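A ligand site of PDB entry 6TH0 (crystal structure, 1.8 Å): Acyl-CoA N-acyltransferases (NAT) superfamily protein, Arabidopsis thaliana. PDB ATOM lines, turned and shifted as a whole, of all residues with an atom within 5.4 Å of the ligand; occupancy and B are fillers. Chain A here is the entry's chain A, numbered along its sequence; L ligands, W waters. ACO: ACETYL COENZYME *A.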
ATOM      1  N   ILE A  26      -3.877 -20.507 -30.394  1.00  0.00           N
ATOM      2  CA  ILE A  26      -2.634 -19.865 -29.942  1.00  0.00           C
ATOM      3  C   ILE A  26      -1.655 -20.805 -29.260  1.00  0.00           C
ATOM      4  O   ILE A  26      -0.498 -20.429 -29.048  1.00  0.00           O
ATOM      5  CB  ILE A  26      -2.918 -18.651 -29.035  1.00  0.00           C
ATOM      6  CG1 ILE A  26      -3.275 -19.082 -27.605  1.00  0.00           C
ATOM      7  CG2 ILE A  26      -4.030 -17.752 -29.622  1.00  0.00           C
ATOM      8  CD1 ILE A  26      -3.465 -17.887 -26.674  1.00  0.00           C
ATOM      9  N   PHE A  27      -2.101 -22.008 -28.881  1.00  0.00           N
ATOM     10  CA  PHE A  27      -1.160 -22.865 -28.174  1.00  0.00           C
ATOM     11  C   PHE A  27      -0.589 -23.910 -29.128  1.00  0.00           C
ATOM     12  O   PHE A  27      -1.348 -24.727 -29.675  1.00  0.00           O
ATOM     13  CB  PHE A  27      -1.816 -23.539 -26.979  1.00  0.00           C
ATOM     14  CG  PHE A  27      -0.818 -24.065 -26.008  1.00  0.00           C
ATOM     15  CD1 PHE A  27      -0.173 -23.202 -25.151  1.00  0.00           C
ATOM     16  CD2 PHE A  27      -0.462 -25.399 -26.003  1.00  0.00           C
ATOM     17  CE1 PHE A  27       0.809 -23.677 -24.266  1.00  0.00           C
ATOM     18  CE2 PHE A  27       0.502 -25.870 -25.140  1.00  0.00           C
ATOM     19  CZ  PHE A  27       1.142 -25.000 -24.278  1.00  0.00           C
ATOM     20  N   PRO A  28       0.730 -23.952 -29.308  1.00  0.00           N
ATOM     21  CA  PRO A  28       1.302 -24.800 -30.365  1.00  0.00           C
ATOM     22  C   PRO A  28       1.101 -26.295 -30.169  1.00  0.00           C
ATOM     23  O   PRO A  28       1.088 -27.019 -31.170  1.00  0.00           O
ATOM     24  CB  PRO A  28       2.802 -24.440 -30.327  1.00  0.00           C
ATOM     25  CG  PRO A  28       2.880 -23.171 -29.553  1.00  0.00           C
ATOM     26  CD  PRO A  28       1.766 -23.186 -28.587  1.00  0.00           C
ATOM     27  N   LEU A  98       0.939 -27.231 -17.749  1.00  0.00           N
ATOM     28  CA  LEU A  98       0.700 -27.846 -19.045  1.00  0.00           C
ATOM     29  C   LEU A  98       0.596 -26.780 -20.132  1.00  0.00           C
ATOM     30  O   LEU A  98       1.337 -26.804 -21.115  1.00  0.00           O
ATOM     31  CB  LEU A  98      -0.599 -28.647 -19.015  1.00  0.00           C
ATOM     32  CG  LEU A  98      -0.626 -29.855 -18.049  1.00  0.00           C
ATOM     33  CD1 LEU A  98      -2.061 -30.172 -17.689  1.00  0.00           C
ATOM     34  CD2 LEU A  98      -0.018 -31.030 -18.776  1.00  0.00           C
ATOM     35  N   LEU A 100      -0.412 -22.438 -21.157  1.00  0.00           N
ATOM     36  CA  LEU A 100      -0.512 -21.051 -20.720  1.00  0.00           C
ATOM     37  C   LEU A 100      -0.694 -20.224 -21.977  1.00  0.00           C
ATOM     38  O   LEU A 100       0.001 -20.493 -22.957  1.00  0.00           O
ATOM     39  CB  LEU A 100       0.756 -20.613 -19.971  1.00  0.00           C
ATOM     40  CG  LEU A 100       0.970 -19.136 -19.741  1.00  0.00           C
ATOM     41  CD1 LEU A 100       0.047 -18.637 -18.637  1.00  0.00           C
ATOM     42  CD2 LEU A 100       2.427 -18.856 -19.388  1.00  0.00           C
ATOM     43  N   GLY A 101      -1.633 -19.288 -21.971  1.00  0.00           N
ATOM     44  CA  GLY A 101      -1.840 -18.436 -23.132  1.00  0.00           C
ATOM     45  C   GLY A 101      -2.643 -17.210 -22.769  1.00  0.00           C
ATOM     46  O   GLY A 101      -3.479 -17.242 -21.866  1.00  0.00           O
ATOM     47  N   VAL A 102      -2.417 -16.121 -23.511  1.00  0.00           N
ATOM     48  CA  VAL A 102      -3.181 -14.880 -23.400  1.00  0.00           C
ATOM     49  C   VAL A 102      -3.568 -14.469 -24.821  1.00  0.00           C
ATOM     50  O   VAL A 102      -2.751 -14.604 -25.738  1.00  0.00           O
ATOM     51  CB  VAL A 102      -2.365 -13.783 -22.679  1.00  0.00           C
ATOM     52  CG1 VAL A 102      -3.125 -12.483 -22.623  1.00  0.00           C
ATOM     53  CG2 VAL A 102      -1.940 -14.231 -21.248  1.00  0.00           C
ATOM     54  N   VAL A 103      -4.813 -14.022 -25.024  1.00  0.00           N
ATOM     55  CA  VAL A 103      -5.188 -13.639 -26.379  1.00  0.00           C
ATOM     56  C   VAL A 103      -4.339 -12.442 -26.825  1.00  0.00           C
ATOM     57  O   VAL A 103      -4.011 -11.552 -26.035  1.00  0.00           O
ATOM     58  CB  VAL A 103      -6.684 -13.338 -26.567  1.00  0.00           C
ATOM     59  CG1 VAL A 103      -7.587 -14.501 -26.084  1.00  0.00           C
ATOM     60  CG2 VAL A 103      -7.077 -12.033 -25.930  1.00  0.00           C
ATOM     61  N   TYR A 106      -4.535  -8.875 -25.613  1.00  0.00           N
ATOM     62  CA  TYR A 106      -4.377  -8.636 -24.175  1.00  0.00           C
ATOM     63  C   TYR A 106      -2.943  -8.837 -23.697  1.00  0.00           C
ATOM     64  O   TYR A 106      -2.697  -8.798 -22.487  1.00  0.00           O
ATOM     65  CB  TYR A 106      -5.323  -9.544 -23.373  1.00  0.00           C
ATOM     66  CG  TYR A 106      -6.744  -9.046 -23.298  1.00  0.00           C
ATOM     67  CD1 TYR A 106      -7.648  -9.319 -24.323  1.00  0.00           C
ATOM     68  CD2 TYR A 106      -7.188  -8.310 -22.214  1.00  0.00           C
ATOM     69  CE1 TYR A 106      -8.949  -8.860 -24.267  1.00  0.00           C
ATOM     70  CE2 TYR A 106      -8.485  -7.841 -22.150  1.00  0.00           C
ATOM     71  CZ  TYR A 106      -9.363  -8.120 -23.179  1.00  0.00           C
ATOM     72  OH  TYR A 106     -10.663  -7.661 -23.122  1.00  0.00           O
ATOM     73  N   ARG A 107      -2.001  -9.043 -24.605  1.00  0.00           N
ATOM     74  CA  ARG A 107      -0.639  -9.376 -24.202  1.00  0.00           C
ATOM     75  C   ARG A 107       0.147  -8.149 -23.759  1.00  0.00           C
ATOM     76  O   ARG A 107      -0.207  -7.010 -24.050  1.00  0.00           O
ATOM     77  CB  ARG A 107       0.077 -10.098 -25.338  1.00  0.00           C
ATOM     78  CG  ARG A 107      -0.473 -11.499 -25.523  1.00  0.00           C
ATOM     79  CD  ARG A 107       0.176 -12.219 -26.671  1.00  0.00           C
ATOM     80  NE  ARG A 107      -0.565 -13.428 -26.975  1.00  0.00           N
ATOM     81  CZ  ARG A 107      -0.348 -14.208 -28.018  1.00  0.00           C
ATOM     82  NH1 ARG A 107       0.616 -13.919 -28.876  1.00  0.00           N
ATOM     83  NH2 ARG A 107      -1.099 -15.287 -28.210  1.00  0.00           N
ATOM     84  N   LYS A 108       1.229  -8.399 -23.030  1.00  0.00           N
ATOM     85  CA  LYS A 108       2.124  -7.360 -22.541  1.00  0.00           C
ATOM     86  C   LYS A 108       1.447  -6.472 -21.505  1.00  0.00           C
ATOM     87  O   LYS A 108       1.725  -5.281 -21.417  1.00  0.00           O
ATOM     88  CB  LYS A 108       2.697  -6.513 -23.680  1.00  0.00           C
ATOM     89  CG  LYS A 108       3.439  -7.366 -24.714  1.00  0.00           C
ATOM     90  CD  LYS A 108       4.610  -6.617 -25.311  1.00  0.00           C
ATOM     91  CE  LYS A 108       5.786  -7.577 -25.510  1.00  0.00           C
ATOM     92  NZ  LYS A 108       7.085  -6.878 -25.755  1.00  0.00           N
ATOM     93  N   ARG A 109       0.533  -7.052 -20.716  1.00  0.00           N
ATOM     94  CA  ARG A 109      -0.113  -6.349 -19.619  1.00  0.00           C
ATOM     95  C   ARG A 109       0.110  -7.055 -18.285  1.00  0.00           C
ATOM     96  O   ARG A 109      -0.431  -6.623 -17.268  1.00  0.00           O
ATOM     97  CB  ARG A 109      -1.611  -6.209 -19.906  1.00  0.00           C
ATOM     98  CG  ARG A 109      -1.920  -5.458 -21.194  1.00  0.00           C
ATOM     99  CD  ARG A 109      -3.411  -5.228 -21.399  1.00  0.00           C
ATOM    100  NE  ARG A 109      -3.670  -4.761 -22.765  1.00  0.00           N
ATOM    101  CZ  ARG A 109      -4.874  -4.551 -23.274  1.00  0.00           C
ATOM    102  NH1 ARG A 109      -5.001  -4.130 -24.523  1.00  0.00           N
ATOM    103  NH2 ARG A 109      -5.963  -4.754 -22.538  1.00  0.00           N
ATOM    104  N   GLY A 110       0.930  -8.104 -18.263  1.00  0.00           N
ATOM    105  CA  GLY A 110       1.189  -8.844 -17.041  1.00  0.00           C
ATOM    106  C   GLY A 110       0.203  -9.958 -16.746  1.00  0.00           C
ATOM    107  O   GLY A 110       0.259 -10.527 -15.647  1.00  0.00           O
ATOM    108  N   ILE A 111      -0.675 -10.303 -17.688  1.00  0.00           N
ATOM    109  CA  ILE A 111      -1.675 -11.326 -17.411  1.00  0.00           C
ATOM    110  C   ILE A 111      -1.015 -12.693 -17.267  1.00  0.00           C
ATOM    111  O   ILE A 111      -1.310 -13.449 -16.335  1.00  0.00           O
ATOM    112  CB  ILE A 111      -2.772 -11.307 -18.492  1.00  0.00           C
ATOM    113  CG1 ILE A 111      -3.544  -9.988 -18.396  1.00  0.00           C
ATOM    114  CG2 ILE A 111      -3.735 -12.505 -18.335  1.00  0.00           C
ATOM    115  CD1 ILE A 111      -4.467  -9.718 -19.612  1.00  0.00           C
ATOM    116  N   ALA A 112      -0.099 -13.035 -18.178  1.00  0.00           N
ATOM    117  CA  ALA A 112       0.559 -14.336 -18.084  1.00  0.00           C
ATOM    118  C   ALA A 112       1.364 -14.437 -16.803  1.00  0.00           C
ATOM    119  O   ALA A 112       1.354 -15.478 -16.137  1.00  0.00           O
ATOM    120  CB  ALA A 112       1.461 -14.569 -19.288  1.00  0.00           C
ATOM    121  N   LYS A 113       2.085 -13.379 -16.438  1.00  0.00           N
ATOM    122  CA  LYS A 113       2.784 -13.377 -15.167  1.00  0.00           C
ATOM    123  C   LYS A 113       1.824 -13.637 -14.011  1.00  0.00           C
ATOM    124  O   LYS A 113       2.136 -14.399 -13.095  1.00  0.00           O
ATOM    125  CB  LYS A 113       3.509 -12.039 -14.992  1.00  0.00           C
ATOM    126  CG  LYS A 113       4.285 -11.923 -13.697  1.00  0.00           C
ATOM    127  CD  LYS A 113       5.079 -10.613 -13.668  1.00  0.00           C
ATOM    128  CE  LYS A 113       6.148 -10.626 -12.584  1.00  0.00           C
ATOM    129  NZ  LYS A 113       5.560 -10.658 -11.216  1.00  0.00           N
ATOM    130  N   LEU A 134       7.764 -27.182 -15.602  1.00  0.00           N
ATOM    131  CA  LEU A 134       7.137 -27.156 -16.914  1.00  0.00           C
ATOM    132  C   LEU A 134       8.216 -27.262 -17.972  1.00  0.00           C
ATOM    133  O   LEU A 134       9.415 -27.185 -17.672  1.00  0.00           O
ATOM    134  CB  LEU A 134       6.310 -25.879 -17.090  1.00  0.00           C
ATOM    135  CG  LEU A 134       7.199 -24.633 -17.172  1.00  0.00           C
ATOM    136  CD1 LEU A 134       6.507 -23.616 -18.033  1.00  0.00           C
ATOM    137  CD2 LEU A 134       7.547 -24.035 -15.801  1.00  0.00           C
ATOM    138  N   HIS A 135       7.779 -27.399 -19.206  1.00  0.00           N
ATOM    139  CA  HIS A 135       8.657 -27.382 -20.358  1.00  0.00           C
ATOM    140  C   HIS A 135       8.234 -26.245 -21.279  1.00  0.00           C
ATOM    141  O   HIS A 135       7.044 -26.009 -21.479  1.00  0.00           O
ATOM    142  CB  HIS A 135       8.641 -28.716 -21.120  1.00  0.00           C
ATOM    143  CG  HIS A 135       9.174 -29.866 -20.322  1.00  0.00           C
ATOM    144  ND1 HIS A 135       8.388 -30.642 -19.493  1.00  0.00           N
ATOM    145  CD2 HIS A 135      10.422 -30.381 -20.258  1.00  0.00           C
ATOM    146  CE1 HIS A 135       9.137 -31.581 -18.950  1.00  0.00           C
ATOM    147  NE2 HIS A 135      10.372 -31.448 -19.386  1.00  0.00           N
ATOM    148  N   VAL A 136       9.219 -25.532 -21.803  1.00  0.00           N
ATOM    149  CA  VAL A 136       9.014 -24.431 -22.726  1.00  0.00           C
ATOM    150  C   VAL A 136       9.637 -24.814 -24.057  1.00  0.00           C
ATOM    151  O   VAL A 136      10.749 -25.347 -24.108  1.00  0.00           O
ATOM    152  CB  VAL A 136       9.655 -23.138 -22.170  1.00  0.00           C
ATOM    153  CG1 VAL A 136       9.465 -21.981 -23.113  1.00  0.00           C
ATOM    154  CG2 VAL A 136       9.101 -22.829 -20.770  1.00  0.00           C
ATOM    155  N   ILE A 137       8.931 -24.524 -25.156  1.00  0.00           N
ATOM    156  CA  ILE A 137       9.549 -24.729 -26.453  1.00  0.00           C
ATOM    157  C   ILE A 137      10.796 -23.871 -26.515  1.00  0.00           C
ATOM    158  O   ILE A 137      10.768 -22.690 -26.159  1.00  0.00           O
ATOM    159  CB  ILE A 137       8.563 -24.338 -27.564  1.00  0.00           C
ATOM    160  CG1 ILE A 137       7.388 -25.320 -27.596  1.00  0.00           C
ATOM    161  CG2 ILE A 137       9.285 -24.275 -28.896  1.00  0.00           C
ATOM    162  CD1 ILE A 137       6.276 -24.895 -28.569  1.00  0.00           C
ATOM    163  N   ASN A 140      11.076 -20.311 -28.056  1.00  0.00           N
ATOM    164  CA  ASN A 140      10.061 -19.352 -27.594  1.00  0.00           C
ATOM    165  C   ASN A 140      10.706 -18.416 -26.581  1.00  0.00           C
ATOM    166  O   ASN A 140      10.575 -18.568 -25.367  1.00  0.00           O
ATOM    167  CB  ASN A 140       8.863 -20.084 -27.009  1.00  0.00           C
ATOM    168  CG  ASN A 140       7.677 -19.164 -26.728  1.00  0.00           C
ATOM    169  OD1 ASN A 140       7.820 -17.953 -26.588  1.00  0.00           O
ATOM    170  ND2 ASN A 140       6.498 -19.748 -26.609  1.00  0.00           N
ATOM    171  N   PRO A 142      10.003 -15.219 -25.727  1.00  0.00           N
ATOM    172  CA  PRO A 142       9.124 -14.532 -24.768  1.00  0.00           C
ATOM    173  C   PRO A 142       8.759 -15.392 -23.576  1.00  0.00           C
ATOM    174  O   PRO A 142       8.749 -14.896 -22.433  1.00  0.00           O
ATOM    175  CB  PRO A 142       7.906 -14.172 -25.626  1.00  0.00           C
ATOM    176  CG  PRO A 142       8.499 -13.965 -26.987  1.00  0.00           C
ATOM    177  CD  PRO A 142       9.583 -14.997 -27.128  1.00  0.00           C
ATOM    178  N   ALA A 143       8.495 -16.677 -23.798  1.00  0.00           N
ATOM    179  CA  ALA A 143       8.179 -17.585 -22.705  1.00  0.00           C
ATOM    180  C   ALA A 143       9.383 -17.786 -21.801  1.00  0.00           C
ATOM    181  O   ALA A 143       9.244 -17.766 -20.568  1.00  0.00           O
ATOM    182  CB  ALA A 143       7.703 -18.923 -23.269  1.00  0.00           C
ATOM    183  N   ARG A 145      11.849 -15.648 -21.265  1.00  0.00           N
ATOM    184  CA  ARG A 145      11.992 -14.433 -20.469  1.00  0.00           C
ATOM    185  C   ARG A 145      10.945 -14.358 -19.359  1.00  0.00           C
ATOM    186  O   ARG A 145      11.228 -13.859 -18.253  1.00  0.00           O
ATOM    187  CB  ARG A 145      11.915 -13.188 -21.357  1.00  0.00           C
ATOM    188  CG  ARG A 145      13.035 -13.073 -22.372  1.00  0.00           C
ATOM    189  CD  ARG A 145      13.114 -11.681 -23.023  1.00  0.00           C
ATOM    190  NE  ARG A 145      11.879 -11.285 -23.692  1.00  0.00           N
ATOM    191  CZ  ARG A 145      11.597 -11.533 -24.973  1.00  0.00           C
ATOM    192  NH1 ARG A 145      10.444 -11.133 -25.487  1.00  0.00           N
ATOM    193  NH2 ARG A 145      12.459 -12.192 -25.734  1.00  0.00           N
ATOM    194  N   LEU A 146       9.720 -14.801 -19.648  1.00  0.00           N
ATOM    195  CA  LEU A 146       8.636 -14.745 -18.667  1.00  0.00           C
ATOM    196  C   LEU A 146       8.928 -15.639 -17.461  1.00  0.00           C
ATOM    197  O   LEU A 146       8.788 -15.224 -16.306  1.00  0.00           O
ATOM    198  CB  LEU A 146       7.323 -15.176 -19.335  1.00  0.00           C
ATOM    199  CG  LEU A 146       6.060 -15.312 -18.474  1.00  0.00           C
ATOM    200  CD1 LEU A 146       5.716 -13.999 -17.818  1.00  0.00           C
ATOM    201  CD2 LEU A 146       4.893 -15.832 -19.323  1.00  0.00           C
ATOM    202  N   TYR A 147       9.317 -16.875 -17.708  1.00  0.00           N
ATOM    203  CA  TYR A 147       9.528 -17.763 -16.573  1.00  0.00           C
ATOM    204  C   TYR A 147      10.768 -17.344 -15.789  1.00  0.00           C
ATOM    205  O   TYR A 147      10.768 -17.399 -14.550  1.00  0.00           O
ATOM    206  CB  TYR A 147       9.580 -19.210 -17.057  1.00  0.00           C
ATOM    207  CG  TYR A 147       8.186 -19.769 -17.307  1.00  0.00           C
ATOM    208  CD1 TYR A 147       7.353 -20.093 -16.250  1.00  0.00           C
ATOM    209  CD2 TYR A 147       7.696 -19.917 -18.601  1.00  0.00           C
ATOM    210  CE1 TYR A 147       6.081 -20.576 -16.456  1.00  0.00           C
ATOM    211  CE2 TYR A 147       6.416 -20.399 -18.818  1.00  0.00           C
ATOM    212  CZ  TYR A 147       5.621 -20.725 -17.737  1.00  0.00           C
ATOM    213  OH  TYR A 147       4.355 -21.221 -17.940  1.00  0.00           O
ATOM    214  N   ARG A 149      11.695 -14.302 -15.425  1.00  0.00           N
ATOM    215  CA  ARG A 149      11.256 -13.132 -14.676  1.00  0.00           C
ATOM    216  C   ARG A 149      10.525 -13.539 -13.405  1.00  0.00           C
ATOM    217  O   ARG A 149      10.588 -12.831 -12.390  1.00  0.00           O
ATOM    218  CB  ARG A 149      10.312 -12.295 -15.536  1.00  0.00           C
ATOM    219  CG  ARG A 149       9.916 -10.953 -14.971  1.00  0.00           C
ATOM    220  CD  ARG A 149       9.027 -10.211 -15.979  1.00  0.00           C
ATOM    221  NE  ARG A 149       9.657 -10.008 -17.279  1.00  0.00           N
ATOM    222  CZ  ARG A 149       9.214 -10.509 -18.427  1.00  0.00           C
ATOM    223  NH1 ARG A 149       8.113 -11.259 -18.458  1.00  0.00           N
ATOM    224  NH2 ARG A 149       9.872 -10.256 -19.551  1.00  0.00           N
ATOM    225  N   TYR A 162       8.957 -31.955 -28.258  1.00  0.00           N
ATOM    226  CA  TYR A 162       7.691 -31.548 -28.857  1.00  0.00           C
ATOM    227  C   TYR A 162       7.596 -31.971 -30.319  1.00  0.00           C
ATOM    228  O   TYR A 162       8.600 -32.046 -31.027  1.00  0.00           O
ATOM    229  CB  TYR A 162       7.524 -30.029 -28.759  1.00  0.00           C
ATOM    230  CG  TYR A 162       7.270 -29.521 -27.357  1.00  0.00           C
ATOM    231  CD1 TYR A 162       6.171 -29.950 -26.643  1.00  0.00           C
ATOM    232  CD2 TYR A 162       8.109 -28.590 -26.762  1.00  0.00           C
ATOM    233  CE1 TYR A 162       5.913 -29.479 -25.370  1.00  0.00           C
ATOM    234  CE2 TYR A 162       7.849 -28.101 -25.475  1.00  0.00           C
ATOM    235  CZ  TYR A 162       6.740 -28.558 -24.795  1.00  0.00           C
ATOM    236  OH  TYR A 162       6.462 -28.112 -23.528  1.00  0.00           O
HETATM  237  N1A ACO L   1       3.704  -2.297 -19.927  1.00  0.00           N
HETATM  238  C2A ACO L   1       4.559  -2.750 -20.909  1.00  0.00           C
HETATM  239  N3A ACO L   1       5.103  -3.963 -21.125  1.00  0.00           N
HETATM  240  C4A ACO L   1       4.704  -4.876 -20.149  1.00  0.00           C
HETATM  241  C5A ACO L   1       3.830  -4.557 -19.068  1.00  0.00           C
HETATM  242  C6A ACO L   1       3.345  -3.235 -18.995  1.00  0.00           C
HETATM  243  N6A ACO L   1       2.507  -2.869 -17.978  1.00  0.00           N
HETATM  244  N7A ACO L   1       3.610  -5.673 -18.246  1.00  0.00           N
HETATM  245  C8A ACO L   1       4.336  -6.644 -18.830  1.00  0.00           C
HETATM  246  N9A ACO L   1       5.024  -6.219 -19.975  1.00  0.00           N
HETATM  247  C1B ACO L   1       5.900  -7.001 -20.830  1.00  0.00           C
HETATM  248  C2B ACO L   1       6.830  -8.040 -20.048  1.00  0.00           C
HETATM  249  O2B ACO L   1       7.922  -7.399 -19.534  1.00  0.00           O
HETATM  250  C3B ACO L   1       7.187  -8.871 -21.368  1.00  0.00           C
HETATM  251  O3B ACO L   1       8.027  -8.079 -22.046  1.00  0.00           O
HETATM  252  P3B ACO L   1       9.266  -9.024 -23.036  1.00  0.00           P
HETATM  253  O7A ACO L   1       8.291  -9.495 -24.086  1.00  0.00           O
HETATM  254  O8A ACO L   1      10.276  -7.971 -23.440  1.00  0.00           O
HETATM  255  O9A ACO L   1       9.664 -10.064 -22.017  1.00  0.00           O
HETATM  256  C4B ACO L   1       5.791  -8.991 -22.064  1.00  0.00           C
HETATM  257  O4B ACO L   1       5.076  -7.751 -21.765  1.00  0.00           O
HETATM  258  C5B ACO L   1       5.026 -10.245 -21.611  1.00  0.00           C
HETATM  259  O5B ACO L   1       4.907 -10.309 -20.229  1.00  0.00           O
HETATM  260  P1A ACO L   1       3.345 -10.671 -19.842  1.00  0.00           P
HETATM  261  O1A ACO L   1       2.457  -9.588 -20.327  1.00  0.00           O
HETATM  262  O2A ACO L   1       3.337 -11.106 -18.401  1.00  0.00           O
HETATM  263  O3A ACO L   1       2.837 -12.056 -20.667  1.00  0.00           O
HETATM  264  P2A ACO L   1       1.644 -11.861 -21.689  1.00  0.00           P
HETATM  265  O4A ACO L   1       0.328 -11.730 -21.003  1.00  0.00           O
HETATM  266  O5A ACO L   1       1.962 -10.987 -22.871  1.00  0.00           O
HETATM  267  O6A ACO L   1       1.479 -13.432 -22.405  1.00  0.00           O
HETATM  268  CBP ACO L   1       2.499 -15.412 -23.340  1.00  0.00           C
HETATM  269  CCP ACO L   1       2.723 -14.054 -22.535  1.00  0.00           C
HETATM  270  CDP ACO L   1       1.701 -16.334 -22.447  1.00  0.00           C
HETATM  271  CEP ACO L   1       3.840 -16.037 -23.698  1.00  0.00           C
HETATM  272  CAP ACO L   1       1.696 -15.012 -24.607  1.00  0.00           C
HETATM  273  OAP ACO L   1       2.525 -14.319 -25.535  1.00  0.00           O
HETATM  274  C9P ACO L   1       1.080 -16.182 -25.358  1.00  0.00           C
HETATM  275  O9P ACO L   1      -0.067 -16.516 -25.149  1.00  0.00           O
HETATM  276  N8P ACO L   1       1.830 -16.802 -26.342  1.00  0.00           N
HETATM  277  C7P ACO L   1       1.291 -17.952 -27.140  1.00  0.00           C
HETATM  278  C6P ACO L   1       1.092 -19.155 -26.258  1.00  0.00           C
HETATM  279  C5P ACO L   1       2.431 -19.561 -25.760  1.00  0.00           C
HETATM  280  O5P ACO L   1       3.463 -19.502 -26.403  1.00  0.00           O
HETATM  281  N4P ACO L   1       2.470 -20.031 -24.459  1.00  0.00           N
HETATM  282  C3P ACO L   1       3.803 -20.413 -23.981  1.00  0.00           C
HETATM  283  C2P ACO L   1       3.675 -21.497 -22.971  1.00  0.00           C
HETATM  284  S1P ACO L   1       5.390 -21.949 -22.419  1.00  0.00           S
HETATM  285  C   ACO L   1       5.677 -23.203 -23.658  1.00  0.00           C
HETATM  286  O   ACO L   1       6.425 -23.035 -24.597  1.00  0.00           O
HETATM  287  CH3 ACO L   1       4.928 -24.430 -23.537  1.00  0.00           C
HETATM  288  O   HOH W   1       8.105 -12.172 -21.749  1.00  0.00           O
HETATM  289  O   HOH W   2       3.949 -19.629 -29.122  1.00  0.00           O
HETATM  290  O   HOH W   3       5.697 -10.429 -17.306  1.00  0.00           O
HETATM  291  O   HOH W   4       3.467 -11.600 -25.040  1.00  0.00           O
HETATM  292  O   HOH W   5      -0.819  -9.509 -20.613  1.00  0.00           O
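The guanidinium group (NH2) of Arg 149 lies within salt-bridge range of an oxygen (O9A) of the ligand. O5A of the ligand is in hydrogen-bond range of N of Lys 108 (2.7 Å). An oxygen (O7A) of the ligand lies within salt-bridge range of the side-chain amino group (NZ) of Lys 108, 3.3 Å away. N of Val 102 lies within hydrogen-bond range of O9P of the ligand. The backbone carbonyl oxygen (O) of Leu 100 lies within hydrogen-bond range of a nitrogen (N4P) of the ligand, 2.9 Å away. The backbone NH (N) of Gly 110 lies within hydrogen-bond range of an oxygen (O1A) of the ligand (3.0 Å). N of Ile 137 is in hydrogen-bond range of O of the ligand, at 3.0 Å. The guanidinium group (NE) of Arg 145 lies within salt-bridge range of an oxygen (O9A) of the ligand (3.0 Å). O5P of the ligand is in hydrogen-bond range of ND2 of Asn 140 (3.1 Å). O4A of the ligand sits at hydrogen-bond distance from N of Ala 112 (3.1 Å). N of Arg 109 sits at hydrogen-bond distance from O1A of the ligand (3.2 Å). The guanidinium group (NH2) of Arg 107 sits at hydrogen-bond distance from an oxygen (O9P) of the ligand, at 3.5 Å. An oxygen (O2A) of the ligand is in hydrogen-bond range of the backbone NH (N) of Lys 113, at 3.3 Å.
The backbone carbonyl oxygen of Val 102 lies within hydrogen-bond range of the guanidinium group of Arg 107, 2.8 Å away. N of Ala 143 lies within hydrogen-bond range of OD1 of Asn 140, 3.1 Å away. O of His 135 lies within hydrogen-bond range of OH of Tyr 162 (3.0 Å).
Merely in contact with the ligand: Ile 26 (3.5 Å), Phe 27 (3.8 Å), Gly 101 (3.3 Å), Ile 111 (3.7 Å), His 135 (3.3 Å), Val 136 (3.5 Å), Ala 143 (3.9 Å), Leu 146 (3.8 Å) and Tyr 162 (3.99 Å). Along chain A the residues within 4 Å of the ligand span positions 26 to 162. The nearest printed residue that does not touch the ligand is Tyr 147 (4.1 Å).
Water W1 lies within hydrogen-bond range of O9A of the ligand (2.6 Å), O of Pro 142 (2.9 Å) and NH2 of Arg 149 (3.4 Å). Water W3 bridges an oxygen (O2A) of the ligand (2.7 Å) and the guanidinium group (NH1) of Arg 149 (2.8 Å).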
